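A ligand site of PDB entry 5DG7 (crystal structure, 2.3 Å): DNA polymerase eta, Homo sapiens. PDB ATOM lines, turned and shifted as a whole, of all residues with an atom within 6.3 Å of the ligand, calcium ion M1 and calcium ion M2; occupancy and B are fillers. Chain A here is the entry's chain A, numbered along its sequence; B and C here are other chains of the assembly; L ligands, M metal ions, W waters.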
ATOM      1  N   ASP A  16      -3.834   1.874 -17.736  1.00  0.00           N
ATOM      2  CA  ASP A  16      -3.099   2.774 -16.862  1.00  0.00           C
ATOM      3  C   ASP A  16      -1.845   3.375 -17.515  1.00  0.00           C
ATOM      4  O   ASP A  16      -0.942   2.648 -17.917  1.00  0.00           O
ATOM      5  CB  ASP A  16      -2.697   2.066 -15.575  1.00  0.00           C
ATOM      6  CG  ASP A  16      -1.787   2.914 -14.726  1.00  0.00           C
ATOM      7  OD1 ASP A  16      -2.293   3.750 -13.983  1.00  0.00           O
ATOM      8  OD2 ASP A  16      -0.560   2.807 -14.840  1.00  0.00           O
ATOM      9  N   MET A  17      -1.777   4.706 -17.551  1.00  0.00           N
ATOM     10  CA  MET A  17      -0.674   5.410 -18.191  1.00  0.00           C
ATOM     11  C   MET A  17       0.638   5.198 -17.447  1.00  0.00           C
ATOM     12  O   MET A  17       0.692   5.281 -16.222  1.00  0.00           O
ATOM     13  CB  MET A  17      -0.976   6.926 -18.277  1.00  0.00           C
ATOM     14  CG  MET A  17      -2.374   7.254 -18.823  1.00  0.00           C
ATOM     15  SD  MET A  17      -2.670   6.614 -20.484  1.00  0.00           S
ATOM     16  CE  MET A  17      -1.390   7.425 -21.409  1.00  0.00           C
ATOM     17  N   ASP A  18       1.698   4.896 -18.201  1.00  0.00           N
ATOM     18  CA  ASP A  18       3.026   4.706 -17.640  1.00  0.00           C
ATOM     19  C   ASP A  18       3.589   6.039 -17.168  1.00  0.00           C
ATOM     20  O   ASP A  18       3.499   7.031 -17.899  1.00  0.00           O
ATOM     21  CB  ASP A  18       3.968   4.046 -18.656  1.00  0.00           C
ATOM     22  CG  ASP A  18       3.517   2.653 -19.066  1.00  0.00           C
ATOM     23  OD1 ASP A  18       2.843   1.962 -18.268  1.00  0.00           O
ATOM     24  OD2 ASP A  18       3.820   2.235 -20.199  1.00  0.00           O
ATOM     25  N   CYS A  19       4.050   6.040 -15.921  1.00  0.00           N
ATOM     26  CA  CYS A  19       4.635   7.188 -15.188  1.00  0.00           C
ATOM     27  C   CYS A  19       4.064   8.515 -15.742  1.00  0.00           C
ATOM     28  O   CYS A  19       4.752   9.248 -16.373  1.00  0.00           O
ATOM     29  CB  CYS A  19       6.154   7.134 -15.331  1.00  0.00           C
ATOM     30  SG  CYS A  19       6.861   7.009 -16.976  1.00  0.00           S
ATOM     31  N   PHE A  20       2.788   8.729 -15.502  1.00  0.00           N
ATOM     32  CA  PHE A  20       1.984   9.653 -16.297  1.00  0.00           C
ATOM     33  C   PHE A  20       2.466  11.110 -16.291  1.00  0.00           C
ATOM     34  O   PHE A  20       2.632  11.687 -17.358  1.00  0.00           O
ATOM     35  CB  PHE A  20       0.524   9.585 -15.851  1.00  0.00           C
ATOM     36  CG  PHE A  20      -0.388  10.462 -16.644  1.00  0.00           C
ATOM     37  CD1 PHE A  20      -0.406  10.388 -18.033  1.00  0.00           C
ATOM     38  CD2 PHE A  20      -1.219  11.368 -16.020  1.00  0.00           C
ATOM     39  CE1 PHE A  20      -1.232  11.215 -18.775  1.00  0.00           C
ATOM     40  CE2 PHE A  20      -2.067  12.197 -16.762  1.00  0.00           C
ATOM     41  CZ  PHE A  20      -2.071  12.124 -18.155  1.00  0.00           C
ATOM     42  N   PHE A  21       2.699  11.711 -15.117  1.00  0.00           N
ATOM     43  CA  PHE A  21       3.137  13.120 -15.099  1.00  0.00           C
ATOM     44  C   PHE A  21       4.503  13.261 -15.778  1.00  0.00           C
ATOM     45  O   PHE A  21       4.765  14.261 -16.449  1.00  0.00           O
ATOM     46  CB  PHE A  21       3.204  13.702 -13.678  1.00  0.00           C
ATOM     47  CG  PHE A  21       1.863  13.911 -13.010  1.00  0.00           C
ATOM     48  CD1 PHE A  21       0.699  13.305 -13.483  1.00  0.00           C
ATOM     49  CD2 PHE A  21       1.774  14.729 -11.891  1.00  0.00           C
ATOM     50  CE1 PHE A  21      -0.537  13.493 -12.840  1.00  0.00           C
ATOM     51  CE2 PHE A  21       0.548  14.932 -11.234  1.00  0.00           C
ATOM     52  CZ  PHE A  21      -0.617  14.308 -11.717  1.00  0.00           C
ATOM     53  N   VAL A  22       5.376  12.257 -15.628  1.00  0.00           N
ATOM     54  CA  VAL A  22       6.677  12.278 -16.306  1.00  0.00           C
ATOM     55  C   VAL A  22       6.517  12.302 -17.818  1.00  0.00           C
ATOM     56  O   VAL A  22       7.122  13.130 -18.499  1.00  0.00           O
ATOM     57  CB  VAL A  22       7.555  11.104 -15.898  1.00  0.00           C
ATOM     58  CG1 VAL A  22       8.696  10.916 -16.888  1.00  0.00           C
ATOM     59  CG2 VAL A  22       8.103  11.306 -14.472  1.00  0.00           C
ATOM     60  N   GLN A  41       7.212  18.650  -6.910  1.00  0.00           N
ATOM     61  CA  GLN A  41       6.493  19.858  -6.575  1.00  0.00           C
ATOM     62  C   GLN A  41       7.192  20.595  -5.449  1.00  0.00           C
ATOM     63  O   GLN A  41       7.719  20.007  -4.498  1.00  0.00           O
ATOM     64  CB  GLN A  41       5.042  19.575  -6.220  1.00  0.00           C
ATOM     65  CG  GLN A  41       4.828  18.450  -5.279  1.00  0.00           C
ATOM     66  CD  GLN A  41       3.372  18.246  -5.039  1.00  0.00           C
ATOM     67  OE1 GLN A  41       2.913  18.242  -3.908  1.00  0.00           O
ATOM     68  NE2 GLN A  41       2.600  18.096  -6.127  1.00  0.00           N
ATOM     69  N   ILE A  51       6.860  13.295  -7.181  1.00  0.00           N
ATOM     70  CA  ILE A  51       5.554  12.645  -7.266  1.00  0.00           C
ATOM     71  C   ILE A  51       5.392  11.709  -8.454  1.00  0.00           C
ATOM     72  O   ILE A  51       4.403  10.978  -8.519  1.00  0.00           O
ATOM     73  CB  ILE A  51       4.395  13.687  -7.325  1.00  0.00           C
ATOM     74  CG1 ILE A  51       4.377  14.434  -8.655  1.00  0.00           C
ATOM     75  CG2 ILE A  51       4.465  14.636  -6.123  1.00  0.00           C
ATOM     76  CD1 ILE A  51       3.302  15.514  -8.696  1.00  0.00           C
ATOM     77  N   ALA A  52       6.331  11.740  -9.403  1.00  0.00           N
ATOM     78  CA  ALA A  52       6.367  10.735 -10.469  1.00  0.00           C
ATOM     79  C   ALA A  52       7.784  10.514 -10.946  1.00  0.00           C
ATOM     80  O   ALA A  52       8.606  11.427 -10.925  1.00  0.00           O
ATOM     81  CB  ALA A  52       5.466  11.131 -11.637  1.00  0.00           C
ATOM     82  N   VAL A  53       8.069   9.289 -11.369  1.00  0.00           N
ATOM     83  CA  VAL A  53       9.430   8.841 -11.601  1.00  0.00           C
ATOM     84  C   VAL A  53       9.507   8.043 -12.894  1.00  0.00           C
ATOM     85  O   VAL A  53       8.788   7.056 -13.030  1.00  0.00           O
ATOM     86  CB  VAL A  53       9.932   7.940 -10.442  1.00  0.00           C
ATOM     87  CG1 VAL A  53      11.389   7.546 -10.666  1.00  0.00           C
ATOM     88  CG2 VAL A  53       9.779   8.643  -9.128  1.00  0.00           C
ATOM     89  N   TYR A  55      10.852   5.305 -15.579  1.00  0.00           N
ATOM     90  CA  TYR A  55      11.349   3.962 -15.328  1.00  0.00           C
ATOM     91  C   TYR A  55      12.872   3.914 -15.340  1.00  0.00           C
ATOM     92  O   TYR A  55      13.455   3.130 -14.605  1.00  0.00           O
ATOM     93  CB  TYR A  55      10.762   2.952 -16.323  1.00  0.00           C
ATOM     94  CG  TYR A  55       9.330   2.589 -15.972  1.00  0.00           C
ATOM     95  CD1 TYR A  55       8.294   3.477 -16.212  1.00  0.00           C
ATOM     96  CD2 TYR A  55       9.033   1.384 -15.361  1.00  0.00           C
ATOM     97  CE1 TYR A  55       6.974   3.164 -15.870  1.00  0.00           C
ATOM     98  CE2 TYR A  55       7.716   1.056 -15.013  1.00  0.00           C
ATOM     99  CZ  TYR A  55       6.690   1.952 -15.269  1.00  0.00           C
ATOM    100  OH  TYR A  55       5.379   1.636 -14.923  1.00  0.00           O
ATOM    101  N   ARG A  58      13.759   4.915 -11.870  1.00  0.00           N
ATOM    102  CA  ARG A  58      13.353   3.844 -10.965  1.00  0.00           C
ATOM    103  C   ARG A  58      14.480   2.812 -10.794  1.00  0.00           C
ATOM    104  O   ARG A  58      14.679   2.278  -9.693  1.00  0.00           O
ATOM    105  CB  ARG A  58      12.069   3.160 -11.460  1.00  0.00           C
ATOM    106  CG  ARG A  58      10.828   4.064 -11.383  1.00  0.00           C
ATOM    107  CD  ARG A  58       9.550   3.346 -11.841  1.00  0.00           C
ATOM    108  NE  ARG A  58       8.512   4.318 -12.167  1.00  0.00           N
ATOM    109  CZ  ARG A  58       7.218   4.045 -12.347  1.00  0.00           C
ATOM    110  NH1 ARG A  58       6.760   2.804 -12.230  1.00  0.00           N
ATOM    111  NH2 ARG A  58       6.384   5.039 -12.630  1.00  0.00           N
ATOM    112  N   ARG A  64       8.629   7.744  -5.577  1.00  0.00           N
ATOM    113  CA  ARG A  64       7.663   8.727  -5.083  1.00  0.00           C
ATOM    114  C   ARG A  64       7.904   9.141  -3.644  1.00  0.00           C
ATOM    115  O   ARG A  64       8.392   8.338  -2.836  1.00  0.00           O
ATOM    116  CB  ARG A  64       6.250   8.136  -5.189  1.00  0.00           C
ATOM    117  CG  ARG A  64       5.215   9.065  -5.724  1.00  0.00           C
ATOM    118  CD  ARG A  64       3.806   8.546  -5.450  1.00  0.00           C
ATOM    119  NE  ARG A  64       3.541   7.207  -5.990  1.00  0.00           N
ATOM    120  CZ  ARG A  64       3.372   6.936  -7.289  1.00  0.00           C
ATOM    121  NH1 ARG A  64       3.466   7.925  -8.192  1.00  0.00           N
ATOM    122  NH2 ARG A  64       3.125   5.695  -7.680  1.00  0.00           N
ATOM    123  N   LEU A  92      -2.353  21.372 -11.174  1.00  0.00           N
ATOM    124  CA  LEU A  92      -2.223  20.142 -11.944  1.00  0.00           C
ATOM    125  C   LEU A  92      -2.910  20.196 -13.284  1.00  0.00           C
ATOM    126  O   LEU A  92      -3.202  19.151 -13.868  1.00  0.00           O
ATOM    127  CB  LEU A  92      -2.790  18.974 -11.120  1.00  0.00           C
ATOM    128  CG  LEU A  92      -2.203  18.879  -9.708  1.00  0.00           C
ATOM    129  CD1 LEU A  92      -2.802  17.681  -8.968  1.00  0.00           C
ATOM    130  CD2 LEU A  92      -0.691  18.777  -9.765  1.00  0.00           C
ATOM    131  N   SER A 116      -9.143   7.355 -12.187  1.00  0.00           N
ATOM    132  CA  SER A 116      -8.212   8.327 -11.642  1.00  0.00           C
ATOM    133  C   SER A 116      -7.794   9.251 -12.778  1.00  0.00           C
ATOM    134  O   SER A 116      -8.307   9.131 -13.888  1.00  0.00           O
ATOM    135  CB  SER A 116      -6.982   7.662 -10.998  1.00  0.00           C
ATOM    136  OG  SER A 116      -6.161   7.035 -11.968  1.00  0.00           O
ATOM    137  N   ILE A 117      -6.858  10.164 -12.513  1.00  0.00           N
ATOM    138  CA  ILE A 117      -6.403  11.077 -13.557  1.00  0.00           C
ATOM    139  C   ILE A 117      -5.776  10.319 -14.745  1.00  0.00           C
ATOM    140  O   ILE A 117      -5.808  10.812 -15.870  1.00  0.00           O
ATOM    141  CB  ILE A 117      -5.394  12.110 -13.011  1.00  0.00           C
ATOM    142  CG1 ILE A 117      -5.299  13.318 -13.954  1.00  0.00           C
ATOM    143  CG2 ILE A 117      -4.032  11.479 -12.739  1.00  0.00           C
ATOM    144  CD1 ILE A 117      -4.634  14.487 -13.315  1.00  0.00           C
ATOM    145  N   ASP A 118      -5.275   9.099 -14.507  1.00  0.00           N
ATOM    146  CA  ASP A 118      -4.626   8.353 -15.600  1.00  0.00           C
ATOM    147  C   ASP A 118      -5.028   6.876 -15.708  1.00  0.00           C
ATOM    148  O   ASP A 118      -4.298   6.078 -16.298  1.00  0.00           O
ATOM    149  CB  ASP A 118      -3.106   8.464 -15.444  1.00  0.00           C
ATOM    150  CG  ASP A 118      -2.540   7.477 -14.430  1.00  0.00           C
ATOM    151  OD1 ASP A 118      -3.263   7.079 -13.487  1.00  0.00           O
ATOM    152  OD2 ASP A 118      -1.363   7.095 -14.599  1.00  0.00           O
ATOM    153  N   GLU A 119      -6.172   6.501 -15.129  1.00  0.00           N
ATOM    154  CA  GLU A 119      -6.694   5.133 -15.265  1.00  0.00           C
ATOM    155  C   GLU A 119      -8.162   5.128 -15.678  1.00  0.00           C
ATOM    156  O   GLU A 119      -8.951   5.949 -15.199  1.00  0.00           O
ATOM    157  CB  GLU A 119      -6.562   4.362 -13.955  1.00  0.00           C
ATOM    158  CG  GLU A 119      -5.188   4.410 -13.335  1.00  0.00           C
ATOM    159  CD  GLU A 119      -5.058   3.433 -12.193  1.00  0.00           C
ATOM    160  OE1 GLU A 119      -6.116   3.065 -11.623  1.00  0.00           O
ATOM    161  OE2 GLU A 119      -3.921   3.015 -11.885  1.00  0.00           O
ATOM    162  N   LYS A 234       4.653  -4.137 -16.865  1.00  0.00           N
ATOM    163  CA  LYS A 234       4.738  -2.695 -17.039  1.00  0.00           C
ATOM    164  C   LYS A 234       6.194  -2.383 -17.325  1.00  0.00           C
ATOM    165  O   LYS A 234       7.063  -3.109 -16.849  1.00  0.00           O
ATOM    166  CB  LYS A 234       4.268  -1.951 -15.777  1.00  0.00           C
ATOM    167  CG  LYS A 234       2.830  -1.446 -15.751  1.00  0.00           C
ATOM    168  CD  LYS A 234       2.665  -0.454 -14.577  1.00  0.00           C
ATOM    169  CE  LYS A 234       1.384   0.395 -14.641  1.00  0.00           C
ATOM    170  NZ  LYS A 234       1.398   1.531 -15.642  1.00  0.00           N
ATOM    171  N   PRO A 235       6.486  -1.326 -18.102  1.00  0.00           N
ATOM    172  CA  PRO A 235       5.643  -0.399 -18.854  1.00  0.00           C
ATOM    173  C   PRO A 235       5.342  -0.879 -20.286  1.00  0.00           C
ATOM    174  O   PRO A 235       5.880  -1.892 -20.706  1.00  0.00           O
ATOM    175  CB  PRO A 235       6.505   0.867 -18.911  1.00  0.00           C
ATOM    176  CG  PRO A 235       7.914   0.289 -19.066  1.00  0.00           C
ATOM    177  CD  PRO A 235       7.911  -0.930 -18.162  1.00  0.00           C
ATOM    178  P    DT B   8      -3.657   2.468  -6.650  1.00  0.00           P
ATOM    179  OP1  DT B   8      -3.417   1.358  -7.611  1.00  0.00           O
ATOM    180  OP2  DT B   8      -2.713   2.713  -5.540  1.00  0.00           O
ATOM    181  O5'  DT B   8      -3.776   3.874  -7.431  1.00  0.00           O
ATOM    182  C5'  DT B   8      -4.830   4.116  -8.361  1.00  0.00           C
ATOM    183  C4'  DT B   8      -4.723   5.521  -8.920  1.00  0.00           C
ATOM    184  O4'  DT B   8      -4.919   6.494  -7.850  1.00  0.00           O
ATOM    185  C3'  DT B   8      -3.374   5.852  -9.564  1.00  0.00           C
ATOM    186  O3'  DT B   8      -3.566   6.664 -10.749  1.00  0.00           O
ATOM    187  C2'  DT B   8      -2.657   6.639  -8.466  1.00  0.00           C
ATOM    188  C1'  DT B   8      -3.814   7.363  -7.785  1.00  0.00           C
ATOM    189  N1   DT B   8      -3.543   7.669  -6.345  1.00  0.00           N
ATOM    190  C2   DT B   8      -3.565   8.999  -5.916  1.00  0.00           C
ATOM    191  O2   DT B   8      -3.809   9.941  -6.649  1.00  0.00           O
ATOM    192  N3   DT B   8      -3.305   9.173  -4.587  1.00  0.00           N
ATOM    193  C4   DT B   8      -3.020   8.187  -3.662  1.00  0.00           C
ATOM    194  O4   DT B   8      -2.801   8.453  -2.487  1.00  0.00           O
ATOM    195  C5   DT B   8      -3.004   6.829  -4.184  1.00  0.00           C
ATOM    196  C7   DT B   8      -2.704   5.675  -3.271  1.00  0.00           C
ATOM    197  C6   DT B   8      -3.259   6.646  -5.477  1.00  0.00           C
ATOM    198  P    DT C   3       7.901  13.516   5.264  1.00  0.00           P
ATOM    199  OP1  DT C   3       8.270  13.001   6.602  1.00  0.00           O
ATOM    200  OP2  DT C   3       8.653  13.083   4.048  1.00  0.00           O
ATOM    201  O5'  DT C   3       6.353  13.191   5.022  1.00  0.00           O
ATOM    202  C5'  DT C   3       5.929  12.686   3.758  1.00  0.00           C
ATOM    203  C4'  DT C   3       5.757  13.839   2.782  1.00  0.00           C
ATOM    204  O4'  DT C   3       5.898  13.357   1.407  1.00  0.00           O
ATOM    205  C3'  DT C   3       4.388  14.541   2.833  1.00  0.00           C
ATOM    206  O3'  DT C   3       4.575  15.974   2.817  1.00  0.00           O
ATOM    207  C2'  DT C   3       3.708  14.045   1.562  1.00  0.00           C
ATOM    208  C1'  DT C   3       4.913  13.986   0.637  1.00  0.00           C
ATOM    209  N1   DT C   3       4.677  13.251  -0.645  1.00  0.00           N
ATOM    210  C2   DT C   3       5.068  13.823  -1.847  1.00  0.00           C
ATOM    211  O2   DT C   3       5.630  14.915  -1.928  1.00  0.00           O
ATOM    212  N3   DT C   3       4.791  13.075  -2.957  1.00  0.00           N
ATOM    213  C4   DT C   3       4.171  11.828  -3.001  1.00  0.00           C
ATOM    214  O4   DT C   3       3.955  11.234  -4.048  1.00  0.00           O
ATOM    215  C5   DT C   3       3.776  11.287  -1.709  1.00  0.00           C
ATOM    216  C7   DT C   3       3.110   9.946  -1.639  1.00  0.00           C
ATOM    217  C6   DT C   3       4.042  12.012  -0.618  1.00  0.00           C
ATOM    218  P   EDA C   4       3.323  16.985   2.789  1.00  0.00           P
ATOM    219  OP1 EDA C   4       3.843  18.416   2.956  1.00  0.00           O
ATOM    220  OP2 EDA C   4       2.316  16.590   3.844  1.00  0.00           O
ATOM    221  O5' EDA C   4       2.684  16.831   1.297  1.00  0.00           O
ATOM    222  N9  EDA C   4       0.800  14.814  -2.324  1.00  0.00           N
ATOM    223  C4  EDA C   4       0.665  13.855  -1.405  1.00  0.00           C
ATOM    224  N3  EDA C   4       0.760  13.889  -0.042  1.00  0.00           N
ATOM    225  C2  EDA C   4       0.556  12.745   0.667  1.00  0.00           C
ATOM    226  N1  EDA C   4       0.259  11.578  -0.007  1.00  0.00           N
ATOM    227  C6  EDA C   4       0.162  11.557  -1.353  1.00  0.00           C
ATOM    228  C10 EDA C   4       0.019  10.310   0.441  1.00  0.00           C
ATOM    229  C11 EDA C   4      -0.231   9.517  -0.637  1.00  0.00           C
ATOM    230  N6  EDA C   4      -0.138  10.282  -1.754  1.00  0.00           N
ATOM    231  C5  EDA C   4       0.375  12.709  -2.077  1.00  0.00           C
ATOM    232  N7  EDA C   4       0.343  12.987  -3.412  1.00  0.00           N
ATOM    233  C8  EDA C   4       0.617  14.290  -3.582  1.00  0.00           C
ATOM    234  C2' EDA C   4       0.362  16.864  -1.412  1.00  0.00           C
ATOM    235  C5' EDA C   4       3.530  17.253   0.186  1.00  0.00           C
ATOM    236  C4' EDA C   4       2.715  17.402  -1.093  1.00  0.00           C
ATOM    237  O4' EDA C   4       2.612  16.326  -1.721  1.00  0.00           O
ATOM    238  C1' EDA C   4       1.126  16.211  -2.264  1.00  0.00           C
ATOM    239  C3' EDA C   4       1.239  17.916  -0.833  1.00  0.00           C
ATOM    240  O3' EDA C   4       1.149  19.081  -1.502  1.00  0.00           O
ATOM    241  P    DA C   5      -0.139  20.040  -1.349  1.00  0.00           P
ATOM    242  OP1  DA C   5       0.340  21.369  -1.828  1.00  0.00           O
ATOM    243  OP2  DA C   5      -0.740  19.911  -0.009  1.00  0.00           O
ATOM    244  O5'  DA C   5      -1.133  19.517  -2.490  1.00  0.00           O
ATOM    245  C5'  DA C   5      -0.630  19.375  -3.821  1.00  0.00           C
ATOM    246  C4'  DA C   5      -1.640  18.701  -4.693  1.00  0.00           C
ATOM    247  O4'  DA C   5      -1.651  17.258  -4.451  1.00  0.00           O
ATOM    248  C3'  DA C   5      -3.081  19.177  -4.494  1.00  0.00           C
ATOM    249  O3'  DA C   5      -3.701  19.292  -5.752  1.00  0.00           O
ATOM    250  C2'  DA C   5      -3.700  18.066  -3.660  1.00  0.00           C
ATOM    251  C1'  DA C   5      -2.984  16.838  -4.222  1.00  0.00           C
ATOM    252  N9   DA C   5      -2.951  15.709  -3.303  1.00  0.00           N
ATOM    253  C8   DA C   5      -2.897  15.752  -1.946  1.00  0.00           C
ATOM    254  N7   DA C   5      -2.847  14.571  -1.384  1.00  0.00           N
ATOM    255  C5   DA C   5      -2.902  13.694  -2.453  1.00  0.00           C
ATOM    256  C6   DA C   5      -2.897  12.280  -2.529  1.00  0.00           C
ATOM    257  N6   DA C   5      -2.855  11.483  -1.462  1.00  0.00           N
ATOM    258  N1   DA C   5      -2.943  11.725  -3.759  1.00  0.00           N
ATOM    259  C2   DA C   5      -2.985  12.522  -4.826  1.00  0.00           C
ATOM    260  N3   DA C   5      -2.998  13.852  -4.885  1.00  0.00           N
ATOM    261  C4   DA C   5      -2.963  14.381  -3.649  1.00  0.00           C
HETATM  262  P1  LIG L   1       0.283   6.211 -10.730  1.00  0.00           P
HETATM  263  O1  LIG L   1      -0.448   5.540 -11.804  1.00  0.00           O
HETATM  264  O2  LIG L   1       0.120   5.740  -9.444  1.00  0.00           O
HETATM  265  O3  LIG L   1       1.809   6.287 -11.082  1.00  0.00           O
HETATM  266  P2  LIG L   1       2.607   6.538 -12.409  1.00  0.00           P
HETATM  267  O4  LIG L   1       1.787   6.877 -13.494  1.00  0.00           O
HETATM  268  O5  LIG L   1       3.483   7.596 -12.207  1.00  0.00           O
HETATM  269  O6  LIG L   1       3.475   5.267 -12.663  1.00  0.00           O
HETATM  270  P3  LIG L   1       3.074   3.846 -13.134  1.00  0.00           P
HETATM  271  O7  LIG L   1       1.647   3.824 -13.139  1.00  0.00           O
HETATM  272  O8  LIG L   1       3.655   3.748 -14.397  1.00  0.00           O
HETATM  273  O9  LIG L   1       3.675   3.090 -12.147  1.00  0.00           O
HETATM  274  O10 LIG L   1       0.000   7.720 -10.644  1.00  0.00           O
HETATM  275  C1  LIG L   1      -0.587   8.525 -11.598  1.00  0.00           C
HETATM  276  C2  LIG L   1      -0.053   9.942 -11.531  1.00  0.00           C
HETATM  277  O11 LIG L   1      -0.719  10.734 -10.577  1.00  0.00           O
HETATM  278  C3  LIG L   1       1.414   9.968 -11.235  1.00  0.00           C
HETATM  279  O12 LIG L   1       2.134  10.124 -12.402  1.00  0.00           O
HETATM  280  C4  LIG L   1       1.535  11.164 -10.333  1.00  0.00           C
HETATM  281  C5  LIG L   1       0.172  11.344  -9.693  1.00  0.00           C
HETATM  282  N1  LIG L   1       0.152  10.839  -8.314  1.00  0.00           N
HETATM  283  C6  LIG L   1       0.205  11.738  -7.223  1.00  0.00           C
HETATM  284  O13 LIG L   1       0.245  12.917  -7.453  1.00  0.00           O
HETATM  285  N2  LIG L   1       0.208  11.321  -5.963  1.00  0.00           N
HETATM  286  C7  LIG L   1       0.143  10.050  -5.666  1.00  0.00           C
HETATM  287  O14 LIG L   1       0.153   9.642  -4.525  1.00  0.00           O
HETATM  288  C8  LIG L   1       0.101   9.084  -6.785  1.00  0.00           C
HETATM  289  C9  LIG L   1       0.072   7.634  -6.507  1.00  0.00           C
HETATM  290  C10 LIG L   1       0.112   9.555  -8.060  1.00  0.00           C
HETATM  291 CA    CA M   1      -0.003   5.178 -13.976  1.00  0.00          CA
HETATM  292 CA    CA M   2      -2.730   5.082 -12.115  1.00  0.00          CA
HETATM  293  O   HOH W   1       0.659   2.053 -11.095  1.00  0.00           O
HETATM  294  O   HOH W   2       6.098   7.623 -10.979  1.00  0.00           O
HETATM  295  O   HOH W   3       4.189   3.505  -9.749  1.00  0.00           O
HETATM  296  O   HOH W   4       0.138  15.947  -6.764  1.00  0.00           O
HETATM  297  O   HOH W   5      -3.227  11.119  -9.117  1.00  0.00           O
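O12 of the ligand is in hydrogen-bond range of N of Phe 20, 3.5 Å away.
O8 of the ligand lies within hydrogen-bond range of OH of Tyr 55 (2.8 Å).
N of Cys 19 is in hydrogen-bond range of O8 of the ligand.
The backbone NH (N) of Phe 21 lies within hydrogen-bond range of an oxygen (O12) of the ligand (3.2 Å).
A nitrogen (N2) of the ligand is in hydrogen-bond range of N7 of EDA 4 of chain C, at 3.0 Å.
The guanidinium group (NH2) of Arg 64 lies within salt-bridge range of an oxygen (O2) of the ligand, 3.5 Å away.
The guanidinium group of Arg 58 lies within salt-bridge range of an oxygen (O9) of the ligand, at 3.1 Å.
O8 of the ligand lies within salt-bridge range of NZ of Lys 234, 3.4 Å away.
NE of Arg 58 is in hydrogen-bond range of O of Val 53.
The side-chain carboxylate of Asp 18 is in salt-bridge range of the side-chain amino group of Lys 234.
N3 of DT 8 of chain B sits close to N1 of DA 5 of chain C, 2.7 Å away.
O3' of DT 8 of chain B sits close to the side-chain hydroxyl (OG) of Ser 116 (2.9 Å).
The side-chain amino group of Lys 234 lies within hydrogen-bond range of the backbone carbonyl oxygen of Asp 16 (3.4 Å).
O4' of EDA 4 of chain C sits close to OE1 of Gln 41, 2.9 Å away.
OH of Tyr 55 lies close to NH1 of Arg 58 (3.2 Å).
OG of Ser 116 lies close to N of Asp 118, 3.4 Å away.
Merely in contact with the ligand: Asp 18 (3.4 Å), Ile 51 (3.4 Å), Ala 52 (3.6 Å) and DA 5 of chain C (3.6 Å).
Of the 25 residues printed, 3 come within 4 Å of calcium ion M1.
Ser 116 touches calcium ion M2 (OG to CA, 3.95 Å).
Within 4 Å of calcium ion M2: Asp 16, Ser 116, Asp 118, Glu 119 and DT 8 of chain B.
The nearest printed residue that does not touch calcium ion M2 is Met 17 (5.3 Å).
Calcium ion M1 is bound by an oxygen (O1) of the ligand, an oxygen (O7) of the ligand, the backbone carbonyl oxygen (O) of Met 17, the side-chain carboxylate (OD2) of Asp 118, an oxygen (O4) of the ligand, the side-chain carboxylate (OD2) of Asp 16 and the side-chain carboxylate (OD1) of Asp 16.
Calcium ion M1 has seven donor atoms within binding distance.
O3' of DT 8 of chain B is bound to calcium ion M2, 2.3 Å away.
OD1 of Asp 16 is bound to calcium ion M2.
O1 of the ligand binds calcium ion M2 (2.3 Å).
Calcium ion M2 is bound by the side-chain carboxylate (OE2) of Glu 119 (2.4 Å).
OD1 of Asp 118 is bound to calcium ion M2, 2.5 Å away.
Calcium ion M2 has five donor atoms within binding distance.
Water W3 bridges an oxygen (O9) of the ligand (2.5 Å) and the guanidinium group of Arg 64 (3.2 Å).
Water W2 lies within hydrogen-bond range of the backbone NH (N) of Val 53 (2.6 Å), an oxygen (O5) of the ligand (2.9 Å) and the guanidinium group (NH2) of Arg 58 (3.1 Å).
Water W5 bridges O2 of DT 8 of chain B (2.8 Å) and O11 of the ligand (2.9 Å).
Water W4 lies within hydrogen-bond range of O13 of the ligand (3.1 Å), O4' of DA 5 of chain C (3.2 Å) and NE2 of Gln 41 (3.3 Å).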
